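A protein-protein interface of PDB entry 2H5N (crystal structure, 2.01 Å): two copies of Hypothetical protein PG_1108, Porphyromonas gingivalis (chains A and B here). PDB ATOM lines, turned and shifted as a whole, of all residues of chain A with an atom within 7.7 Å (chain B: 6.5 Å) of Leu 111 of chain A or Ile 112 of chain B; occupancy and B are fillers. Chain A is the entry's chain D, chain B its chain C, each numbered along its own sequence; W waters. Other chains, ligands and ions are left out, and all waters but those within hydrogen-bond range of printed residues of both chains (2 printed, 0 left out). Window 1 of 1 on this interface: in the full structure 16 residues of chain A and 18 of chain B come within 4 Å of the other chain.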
ATOM      1  N   SER A  27      35.830  25.061   7.672  1.00  0.00           N
ATOM      2  CA  SER A  27      35.333  23.797   7.117  1.00  0.00           C
ATOM      3  C   SER A  27      35.352  23.858   5.603  1.00  0.00           C
ATOM      4  O   SER A  27      35.767  22.890   4.936  1.00  0.00           O
ATOM      5  CB  SER A  27      33.907  23.484   7.630  1.00  0.00           C
ATOM      6  OG  SER A  27      33.905  23.297   9.043  1.00  0.00           O
ATOM      7  N   ALA A  31      38.071  21.843   2.754  1.00  0.00           N
ATOM      8  CA  ALA A  31      37.370  20.834   1.968  1.00  0.00           C
ATOM      9  C   ALA A  31      38.255  20.232   0.894  1.00  0.00           C
ATOM     10  O   ALA A  31      38.294  19.008   0.772  1.00  0.00           O
ATOM     11  CB  ALA A  31      36.071  21.412   1.361  1.00  0.00           C
ATOM     12  N   ALA A  69      31.401  21.011  13.899  1.00  0.00           N
ATOM     13  CA  ALA A  69      30.860  21.751  12.756  1.00  0.00           C
ATOM     14  C   ALA A  69      29.330  21.676  12.720  1.00  0.00           C
ATOM     15  O   ALA A  69      28.676  22.649  12.411  1.00  0.00           O
ATOM     16  CB  ALA A  69      31.483  21.271  11.433  1.00  0.00           C
ATOM     17  N   GLU A 105      34.424  26.102  -6.506  1.00  0.00           N
ATOM     18  CA  GLU A 105      34.330  27.040  -5.381  1.00  0.00           C
ATOM     19  C   GLU A 105      32.904  27.519  -5.146  1.00  0.00           C
ATOM     20  O   GLU A 105      32.444  27.638  -3.986  1.00  0.00           O
ATOM     21  CB  GLU A 105      35.259  28.251  -5.538  1.00  0.00           C
ATOM     22  CG  GLU A 105      36.746  27.881  -5.576  1.00  0.00           C
ATOM     23  CD  GLU A 105      37.623  29.043  -6.043  1.00  0.00           C
ATOM     24  OE1 GLU A 105      37.219  29.771  -6.979  1.00  0.00           O
ATOM     25  OE2 GLU A 105      38.711  29.226  -5.456  1.00  0.00           O
ATOM     26  N   LEU A 106      32.208  27.781  -6.244  1.00  0.00           N
ATOM     27  CA  LEU A 106      30.814  28.174  -6.178  1.00  0.00           C
ATOM     28  C   LEU A 106      30.027  27.011  -5.570  1.00  0.00           C
ATOM     29  O   LEU A 106      29.134  27.203  -4.760  1.00  0.00           O
ATOM     30  CB  LEU A 106      30.274  28.544  -7.567  1.00  0.00           C
ATOM     31  CG  LEU A 106      28.799  28.960  -7.617  1.00  0.00           C
ATOM     32  CD1 LEU A 106      28.470  30.092  -6.635  1.00  0.00           C
ATOM     33  CD2 LEU A 106      28.416  29.337  -9.040  1.00  0.00           C
ATOM     34  N   ALA A 107      30.394  25.805  -5.956  1.00  0.00           N
ATOM     35  CA  ALA A 107      29.705  24.597  -5.497  1.00  0.00           C
ATOM     36  C   ALA A 107      29.825  24.457  -3.978  1.00  0.00           C
ATOM     37  O   ALA A 107      28.843  24.133  -3.281  1.00  0.00           O
ATOM     38  CB  ALA A 107      30.261  23.349  -6.220  1.00  0.00           C
ATOM     39  N   LEU A 108      31.023  24.723  -3.464  1.00  0.00           N
ATOM     40  CA  LEU A 108      31.262  24.593  -2.019  1.00  0.00           C
ATOM     41  C   LEU A 108      30.518  25.692  -1.254  1.00  0.00           C
ATOM     42  O   LEU A 108      29.861  25.448  -0.237  1.00  0.00           O
ATOM     43  CB  LEU A 108      32.762  24.629  -1.705  1.00  0.00           C
ATOM     44  CG  LEU A 108      33.605  23.464  -2.231  1.00  0.00           C
ATOM     45  CD1 LEU A 108      35.048  23.875  -2.136  1.00  0.00           C
ATOM     46  CD2 LEU A 108      33.388  22.157  -1.468  1.00  0.00           C
ATOM     47  N   TRP A 109      30.655  26.911  -1.744  1.00  0.00           N
ATOM     48  CA  TRP A 109      29.897  28.010  -1.181  1.00  0.00           C
ATOM     49  C   TRP A 109      28.388  27.685  -1.187  1.00  0.00           C
ATOM     50  O   TRP A 109      27.677  27.916  -0.198  1.00  0.00           O
ATOM     51  CB  TRP A 109      30.262  29.310  -1.900  1.00  0.00           C
ATOM     52  CG  TRP A 109      29.594  30.520  -1.363  1.00  0.00           C
ATOM     53  CD1 TRP A 109      29.206  30.769  -0.065  1.00  0.00           C
ATOM     54  CD2 TRP A 109      29.210  31.667  -2.128  1.00  0.00           C
ATOM     55  NE1 TRP A 109      28.598  32.008   0.004  1.00  0.00           N
ATOM     56  CE2 TRP A 109      28.600  32.580  -1.244  1.00  0.00           C
ATOM     57  CE3 TRP A 109      29.310  32.000  -3.481  1.00  0.00           C
ATOM     58  CZ2 TRP A 109      28.089  33.815  -1.681  1.00  0.00           C
ATOM     59  CZ3 TRP A 109      28.803  33.223  -3.912  1.00  0.00           C
ATOM     60  CH2 TRP A 109      28.212  34.112  -3.016  1.00  0.00           C
ATOM     61  N   THR A 110      27.907  27.115  -2.293  1.00  0.00           N
ATOM     62  CA  THR A 110      26.499  26.739  -2.442  1.00  0.00           C
ATOM     63  C   THR A 110      26.046  25.643  -1.431  1.00  0.00           C
ATOM     64  O   THR A 110      24.964  25.745  -0.783  1.00  0.00           O
ATOM     65  CB  THR A 110      26.200  26.413  -3.937  1.00  0.00           C
ATOM     66  OG1 THR A 110      26.312  27.634  -4.715  1.00  0.00           O
ATOM     67  CG2 THR A 110      24.788  25.805  -4.139  1.00  0.00           C
ATOM     68  N   LEU A 111      26.859  24.609  -1.285  1.00  0.00           N
ATOM     69  CA  LEU A 111      26.561  23.539  -0.335  1.00  0.00           C
ATOM     70  C   LEU A 111      26.454  24.028   1.127  1.00  0.00           C
ATOM     71  O   LEU A 111      25.488  23.709   1.845  1.00  0.00           O
ATOM     72  CB  LEU A 111      27.623  22.448  -0.488  1.00  0.00           C
ATOM     73  CG  LEU A 111      27.388  21.165   0.318  1.00  0.00           C
ATOM     74  CD1 LEU A 111      26.022  20.468  -0.003  1.00  0.00           C
ATOM     75  CD2 LEU A 111      28.563  20.180   0.192  1.00  0.00           C
ATOM     76  N   ILE A 112      27.449  24.799   1.596  1.00  0.00           N
ATOM     77  CA  ILE A 112      27.475  25.209   2.995  1.00  0.00           C
ATOM     78  C   ILE A 112      26.320  26.214   3.222  1.00  0.00           C
ATOM     79  O   ILE A 112      25.648  26.197   4.270  1.00  0.00           O
ATOM     80  CB  ILE A 112      28.902  25.777   3.363  1.00  0.00           C
ATOM     81  CG1 ILE A 112      29.128  25.817   4.868  1.00  0.00           C
ATOM     82  CG2 ILE A 112      29.153  27.183   2.679  1.00  0.00           C
ATOM     83  CD1 ILE A 112      30.587  26.162   5.254  1.00  0.00           C
ATOM     84  N   SER A 113      26.056  27.063   2.225  1.00  0.00           N
ATOM     85  CA  SER A 113      24.913  27.954   2.271  1.00  0.00           C
ATOM     86  C   SER A 113      23.598  27.190   2.454  1.00  0.00           C
ATOM     87  O   SER A 113      22.779  27.569   3.303  1.00  0.00           O
ATOM     88  CB  SER A 113      24.840  28.809   0.995  1.00  0.00           C
ATOM     89  OG  SER A 113      25.804  29.862   1.017  1.00  0.00           O
ATOM     90  N   THR A 114      23.418  26.113   1.681  1.00  0.00           N
ATOM     91  CA  THR A 114      22.190  25.332   1.690  1.00  0.00           C
ATOM     92  C   THR A 114      22.016  24.734   3.069  1.00  0.00           C
ATOM     93  O   THR A 114      20.967  24.912   3.663  1.00  0.00           O
ATOM     94  CB  THR A 114      22.229  24.176   0.637  1.00  0.00           C
ATOM     95  OG1 THR A 114      22.257  24.750  -0.670  1.00  0.00           O
ATOM     96  CG2 THR A 114      20.993  23.270   0.769  1.00  0.00           C
ATOM     97  N   LEU A 115      23.048  24.058   3.577  1.00  0.00           N
ATOM     98  CA  LEU A 115      22.972  23.393   4.889  1.00  0.00           C
ATOM     99  C   LEU A 115      22.763  24.369   6.035  1.00  0.00           C
ATOM    100  O   LEU A 115      22.060  24.035   6.995  1.00  0.00           O
ATOM    101  CB  LEU A 115      24.197  22.511   5.151  1.00  0.00           C
ATOM    102  CG  LEU A 115      24.112  21.039   4.674  1.00  0.00           C
ATOM    103  CD1 LEU A 115      23.824  20.960   3.151  1.00  0.00           C
ATOM    104  CD2 LEU A 115      25.366  20.230   5.005  1.00  0.00           C
ATOM    105  N   CYS A 116      23.368  25.555   5.941  1.00  0.00           N
ATOM    106  CA  CYS A 116      23.178  26.642   6.935  1.00  0.00           C
ATOM    107  C   CYS A 116      21.921  27.486   6.776  1.00  0.00           C
ATOM    108  O   CYS A 116      21.629  28.303   7.651  1.00  0.00           O
ATOM    109  CB  CYS A 116      24.399  27.553   6.998  1.00  0.00           C
ATOM    110  SG  CYS A 116      25.810  26.694   7.691  1.00  0.00           S
ATOM    111  N   GLY A 117      21.172  27.291   5.684  1.00  0.00           N
ATOM    112  CA  GLY A 117      19.925  28.017   5.474  1.00  0.00           C
ATOM    113  C   GLY A 117      20.144  29.463   5.046  1.00  0.00           C
ATOM    114  O   GLY A 117      19.317  30.356   5.334  1.00  0.00           O
ATOM    115  N   LYS B  23      17.978  14.154   1.644  1.00  0.00           N
ATOM    116  CA  LYS B  23      18.164  15.613   1.575  1.00  0.00           C
ATOM    117  C   LYS B  23      19.655  15.960   1.431  1.00  0.00           C
ATOM    118  O   LYS B  23      20.040  16.829   0.630  1.00  0.00           O
ATOM    119  CB  LYS B  23      17.622  16.272   2.837  1.00  0.00           C
ATOM    120  CG  LYS B  23      17.528  17.810   2.756  1.00  0.00           C
ATOM    121  CD  LYS B  23      16.558  18.297   1.706  1.00  0.00           C
ATOM    122  CE  LYS B  23      16.336  19.818   1.919  1.00  0.00           C
ATOM    123  NZ  LYS B  23      15.183  20.400   1.137  1.00  0.00           N
ATOM    124  N   MET B  24      20.490  15.285   2.212  1.00  0.00           N
ATOM    125  CA  MET B  24      21.918  15.513   2.135  1.00  0.00           C
ATOM    126  C   MET B  24      22.445  15.088   0.779  1.00  0.00           C
ATOM    127  O   MET B  24      23.218  15.814   0.166  1.00  0.00           O
ATOM    128  CB  MET B  24      22.660  14.822   3.288  1.00  0.00           C
ATOM    129  CG  MET B  24      22.457  15.532   4.686  1.00  0.00           C
ATOM    130  SD  MET B  24      22.801  17.335   4.858  1.00  0.00           S
ATOM    131  CE  MET B  24      21.410  18.185   4.127  1.00  0.00           C
ATOM    132  N   ALA B  25      22.056  13.904   0.326  1.00  0.00           N
ATOM    133  CA  ALA B  25      22.441  13.446  -1.019  1.00  0.00           C
ATOM    134  C   ALA B  25      21.995  14.407  -2.114  1.00  0.00           C
ATOM    135  O   ALA B  25      22.805  14.757  -2.957  1.00  0.00           O
ATOM    136  CB  ALA B  25      21.934  12.056  -1.291  1.00  0.00           C
ATOM    137  N   SER B  27      21.326  17.623  -1.785  1.00  0.00           N
ATOM    138  CA  SER B  27      22.059  18.902  -1.609  1.00  0.00           C
ATOM    139  C   SER B  27      23.467  18.774  -2.210  1.00  0.00           C
ATOM    140  O   SER B  27      23.968  19.699  -2.895  1.00  0.00           O
ATOM    141  CB  SER B  27      22.161  19.265  -0.127  1.00  0.00           C
ATOM    142  OG  SER B  27      20.863  19.570   0.384  1.00  0.00           O
ATOM    143  N   MET B  28      24.089  17.618  -1.967  1.00  0.00           N
ATOM    144  CA  MET B  28      25.432  17.379  -2.425  1.00  0.00           C
ATOM    145  C   MET B  28      25.485  17.377  -3.942  1.00  0.00           C
ATOM    146  O   MET B  28      26.292  18.119  -4.536  1.00  0.00           O
ATOM    147  CB  MET B  28      25.936  16.026  -1.889  1.00  0.00           C
ATOM    148  CG  MET B  28      27.463  15.804  -2.043  1.00  0.00           C
ATOM    149  SD  MET B  28      28.062  14.146  -1.435  1.00  0.00           S
ATOM    150  CE  MET B  28      26.888  13.132  -2.315  1.00  0.00           C
ATOM    151  N   VAL B  29      24.636  16.548  -4.579  1.00  0.00           N
ATOM    152  CA  VAL B  29      24.746  16.341  -6.060  1.00  0.00           C
ATOM    153  C   VAL B  29      24.254  17.538  -6.864  1.00  0.00           C
ATOM    154  O   VAL B  29      24.579  17.659  -8.051  1.00  0.00           O
ATOM    155  CB  VAL B  29      24.062  15.026  -6.608  1.00  0.00           C
ATOM    156  CG1 VAL B  29      24.718  13.762  -6.030  1.00  0.00           C
ATOM    157  CG2 VAL B  29      22.569  15.020  -6.422  1.00  0.00           C
ATOM    158  N   ALA B  31      24.834  20.693  -5.730  1.00  0.00           N
ATOM    159  CA  ALA B  31      25.713  21.817  -5.278  1.00  0.00           C
ATOM    160  C   ALA B  31      26.372  22.636  -6.414  1.00  0.00           C
ATOM    161  O   ALA B  31      26.450  23.885  -6.364  1.00  0.00           O
ATOM    162  CB  ALA B  31      26.814  21.284  -4.320  1.00  0.00           C
ATOM    163  N   LEU B  91      27.107   8.570   0.804  1.00  0.00           N
ATOM    164  CA  LEU B  91      27.486   9.850   0.186  1.00  0.00           C
ATOM    165  C   LEU B  91      28.766   9.688  -0.654  1.00  0.00           C
ATOM    166  O   LEU B  91      28.871  10.227  -1.752  1.00  0.00           O
ATOM    167  CB  LEU B  91      27.651  10.952   1.247  1.00  0.00           C
ATOM    168  CG  LEU B  91      26.387  11.341   2.038  1.00  0.00           C
ATOM    169  CD1 LEU B  91      26.697  12.368   3.071  1.00  0.00           C
ATOM    170  CD2 LEU B  91      25.245  11.856   1.111  1.00  0.00           C
ATOM    171  N   ALA B 107      36.074  17.029  -2.639  1.00  0.00           N
ATOM    172  CA  ALA B 107      35.958  18.231  -1.833  1.00  0.00           C
ATOM    173  C   ALA B 107      34.513  18.354  -1.286  1.00  0.00           C
ATOM    174  O   ALA B 107      34.308  18.641  -0.108  1.00  0.00           O
ATOM    175  CB  ALA B 107      36.337  19.488  -2.643  1.00  0.00           C
ATOM    176  N   LEU B 108      33.531  18.150  -2.166  1.00  0.00           N
ATOM    177  CA  LEU B 108      32.122  18.191  -1.763  1.00  0.00           C
ATOM    178  C   LEU B 108      31.774  17.094  -0.740  1.00  0.00           C
ATOM    179  O   LEU B 108      31.134  17.371   0.256  1.00  0.00           O
ATOM    180  CB  LEU B 108      31.168  18.179  -2.965  1.00  0.00           C
ATOM    181  CG  LEU B 108      31.208  19.469  -3.792  1.00  0.00           C
ATOM    182  CD1 LEU B 108      30.823  19.163  -5.242  1.00  0.00           C
ATOM    183  CD2 LEU B 108      30.295  20.567  -3.176  1.00  0.00           C
ATOM    184  N   TRP B 109      32.219  15.870  -0.981  1.00  0.00           N
ATOM    185  CA  TRP B 109      31.990  14.795  -0.013  1.00  0.00           C
ATOM    186  C   TRP B 109      32.622  15.074   1.369  1.00  0.00           C
ATOM    187  O   TRP B 109      32.028  14.787   2.431  1.00  0.00           O
ATOM    188  CB  TRP B 109      32.537  13.479  -0.570  1.00  0.00           C
ATOM    189  CG  TRP B 109      32.316  12.251   0.299  1.00  0.00           C
ATOM    190  CD1 TRP B 109      31.259  11.981   1.157  1.00  0.00           C
ATOM    191  CD2 TRP B 109      33.208  11.137   0.397  1.00  0.00           C
ATOM    192  NE1 TRP B 109      31.463  10.737   1.776  1.00  0.00           N
ATOM    193  CE2 TRP B 109      32.651  10.216   1.328  1.00  0.00           C
ATOM    194  CE3 TRP B 109      34.442  10.834  -0.199  1.00  0.00           C
ATOM    195  CZ2 TRP B 109      33.288   9.011   1.659  1.00  0.00           C
ATOM    196  CZ3 TRP B 109      35.062   9.622   0.134  1.00  0.00           C
ATOM    197  CH2 TRP B 109      34.482   8.736   1.052  1.00  0.00           C
ATOM    198  N   THR B 110      33.839  15.601   1.358  1.00  0.00           N
ATOM    199  CA  THR B 110      34.518  15.996   2.598  1.00  0.00           C
ATOM    200  C   THR B 110      33.717  17.103   3.321  1.00  0.00           C
ATOM    201  O   THR B 110      33.455  17.020   4.501  1.00  0.00           O
ATOM    202  CB  THR B 110      35.926  16.466   2.257  1.00  0.00           C
ATOM    203  OG1 THR B 110      36.625  15.367   1.637  1.00  0.00           O
ATOM    204  CG2 THR B 110      36.678  16.896   3.521  1.00  0.00           C
ATOM    205  N   LEU B 111      33.320  18.141   2.597  1.00  0.00           N
ATOM    206  CA  LEU B 111      32.651  19.248   3.265  1.00  0.00           C
ATOM    207  C   LEU B 111      31.346  18.775   3.926  1.00  0.00           C
ATOM    208  O   LEU B 111      31.108  19.071   5.092  1.00  0.00           O
ATOM    209  CB  LEU B 111      32.467  20.475   2.342  1.00  0.00           C
ATOM    210  CG  LEU B 111      31.700  21.673   2.905  1.00  0.00           C
ATOM    211  CD1 LEU B 111      32.422  22.267   4.095  1.00  0.00           C
ATOM    212  CD2 LEU B 111      31.465  22.750   1.809  1.00  0.00           C
ATOM    213  N   ILE B 112      30.521  18.026   3.198  1.00  0.00           N
ATOM    214  CA  ILE B 112      29.209  17.658   3.724  1.00  0.00           C
ATOM    215  C   ILE B 112      29.403  16.709   4.902  1.00  0.00           C
ATOM    216  O   ILE B 112      28.675  16.789   5.877  1.00  0.00           O
ATOM    217  CB  ILE B 112      28.264  17.073   2.601  1.00  0.00           C
ATOM    218  CG1 ILE B 112      26.786  17.086   3.038  1.00  0.00           C
ATOM    219  CG2 ILE B 112      28.748  15.688   2.085  1.00  0.00           C
ATOM    220  CD1 ILE B 112      25.781  16.803   1.898  1.00  0.00           C
ATOM    221  N   SER B 113      30.385  15.812   4.792  1.00  0.00           N
ATOM    222  CA  SER B 113      30.781  14.949   5.907  1.00  0.00           C
ATOM    223  C   SER B 113      31.173  15.748   7.161  1.00  0.00           C
ATOM    224  O   SER B 113      30.728  15.440   8.252  1.00  0.00           O
ATOM    225  CB  SER B 113      31.936  14.032   5.499  1.00  0.00           C
ATOM    226  OG  SER B 113      31.504  13.126   4.503  1.00  0.00           O
ATOM    227  N   THR B 114      31.975  16.795   6.974  1.00  0.00           N
ATOM    228  CA  THR B 114      32.375  17.688   8.048  1.00  0.00           C
ATOM    229  C   THR B 114      31.163  18.336   8.707  1.00  0.00           C
ATOM    230  O   THR B 114      30.998  18.267   9.951  1.00  0.00           O
ATOM    231  CB  THR B 114      33.393  18.769   7.532  1.00  0.00           C
ATOM    232  OG1 THR B 114      34.590  18.096   7.129  1.00  0.00           O
ATOM    233  CG2 THR B 114      33.776  19.761   8.632  1.00  0.00           C
ATOM    234  N   LEU B 115      30.296  18.919   7.881  1.00  0.00           N
ATOM    235  CA  LEU B 115      29.164  19.640   8.417  1.00  0.00           C
ATOM    236  C   LEU B 115      28.193  18.713   9.172  1.00  0.00           C
ATOM    237  O   LEU B 115      27.563  19.133  10.142  1.00  0.00           O
ATOM    238  CB  LEU B 115      28.437  20.443   7.312  1.00  0.00           C
ATOM    239  CG  LEU B 115      29.320  21.390   6.504  1.00  0.00           C
ATOM    240  CD1 LEU B 115      28.603  22.060   5.326  1.00  0.00           C
ATOM    241  CD2 LEU B 115      29.970  22.389   7.465  1.00  0.00           C
ATOM    242  N   CYS B 116      28.066  17.474   8.700  1.00  0.00           N
ATOM    243  CA  CYS B 116      27.123  16.508   9.310  1.00  0.00           C
ATOM    244  C   CYS B 116      27.719  15.657  10.433  1.00  0.00           C
ATOM    245  O   CYS B 116      27.010  14.807  10.968  1.00  0.00           O
ATOM    246  CB  CYS B 116      26.562  15.562   8.236  1.00  0.00           C
ATOM    247  SG  CYS B 116      25.412  16.404   7.144  1.00  0.00           S
ATOM    248  N   GLY B 117      29.007  15.858  10.751  1.00  0.00           N
ATOM    249  CA  GLY B 117      29.671  15.150  11.852  1.00  0.00           C
ATOM    250  C   GLY B 117      30.049  13.707  11.513  1.00  0.00           C
ATOM    251  O   GLY B 117      30.147  12.835  12.398  1.00  0.00           O
ATOM    252  N   LEU B 118      30.271  13.456  10.231  1.00  0.00           N
ATOM    253  CA  LEU B 118      30.567  12.112   9.749  1.00  0.00           C
ATOM    254  C   LEU B 118      32.067  11.831   9.800  1.00  0.00           C
ATOM    255  O   LEU B 118      32.868  12.773   9.724  1.00  0.00           O
ATOM    256  CB  LEU B 118      30.055  11.950   8.297  1.00  0.00           C
ATOM    257  CG  LEU B 118      28.559  12.210   8.067  1.00  0.00           C
ATOM    258  CD1 LEU B 118      28.196  12.075   6.578  1.00  0.00           C
ATOM    259  CD2 LEU B 118      27.665  11.323   8.951  1.00  0.00           C
HETATM  260  O   HOH W   1      35.727  20.244   5.100  1.00  0.00           O
HETATM  261  O   HOH W   2      30.402  18.183  13.213  1.00  0.00           O
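Water W1 lies within hydrogen-bond range of O of Ser 27 of chain A and OG1 of Thr 114 of chain B. Water W2 bridges the backbone NH of Ala 69 of chain A (3.1 Å) and the backbone carbonyl oxygen of Thr 114 of chain B (3.3 Å).
Ser 27 of chain A touches Leu 111 of chain B, and with the chains exchanged Leu 111 of chain A touches Ser 27 of chain B. Ser 27 of chain A touches Thr 114 of chain B, and with the chains exchanged Thr 114 of chain A touches Ser 27 of chain B. Ala 31 of chain A touches Leu 111 of chain B, but with the chains exchanged Leu 111 of chain A does not touch Ala 31 of chain B (4.1 Å). Leu 108 of chain B touches its own counterpart, Leu 108 of chain A. Of the 21 pairs that touch across the chains among the printed residues, 16 have their exchanged pair printed and touching as well.
Of the printed residues of chain B, Leu 111 of chain A touches Ser 27 (3.6 Å), Met 28 (3.96 Å), Leu 108 (3.8 Å) and Ile 112 (3.9 Å). Of the printed residues of chain B, Ile 112 of chain A touches Leu 115 (3.8 Å). Of the printed residues of chain A, Met 24 of chain B touches Leu 115. Val 29 of chain B touches none of the printed residues of chain A. Of the printed residues of chain A, Thr 110 of chain B touches Ala 31. Of chain A, only Leu 111 and Leu 115 come within 4 Å of Ile 112 of chain B. Of the printed residues of chain A, Leu 115 of chain B touches Ile 112 (3.8 Å) and Leu 115 (3.7 Å).
O of Lys 23 of chain B sits at hydrogen-bond distance from OG of Ser 27 of chain B, at 2.9 Å. The side-chain sulfur (SG) of Cys 116 of chain B sits at hydrogen-bond distance from the side-chain sulfur (SD) of Met 24 of chain B, at 3.6 Å. The backbone carbonyl oxygen (O) of Thr 110 of chain B sits at hydrogen-bond distance from the side-chain hydroxyl (OG1) of Thr 114 of chain B (3.1 Å). OG1 of Thr 110 of chain A sits at hydrogen-bond distance from O of Leu 106 of chain A, 2.9 Å away. O of Thr 110 of chain A lies within hydrogen-bond range of OG1 of Thr 114 of chain A (2.9 Å). The side-chain sulfur (SG) of Cys 116 of chain A lies close to the backbone carbonyl oxygen (O) of Ile 112 of chain A, 3.5 Å away.
Hydrophobic or aromatic side chains of chain B within 4 Å of the printed part of chain A: Met 24, Ala 31, Ala 107, Leu 108, Leu 111, Ile 112 and Leu 115. Among the printed residues, 21 pairs touch across the chains. Among the printed residues, no Asp or Glu carboxylate lies within 4 Å of a Lys or Arg side-chain nitrogen of the other chain.
Ser 27 of chain A touches Leu 111 of chain B (O to CD1, 3.5 Å). Ser 27 of chain A touches Thr 114 of chain B. Ala 31 of chain A touches Ala 107 of chain B (O to CA, 3.6 Å). Ala 31 of chain A touches Thr 110 of chain B. CB of Ala 31 of chain A touches CB of Leu 111 of chain B, at 3.9 Å. Ala 107 of chain A touches Leu 108 of chain B. Leu 108 of chain A touches Ala 107 of chain B (CD2 to O, 3.9 Å). O of Leu 108 of chain A touches CD2 of Leu 111 of chain B, 3.7 Å away. Leu 108 of chain B touches Leu 111 of chain A (CD2 to CD2, 3.8 Å). Leu 115 of chain A touches Ile 112 of chain B.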
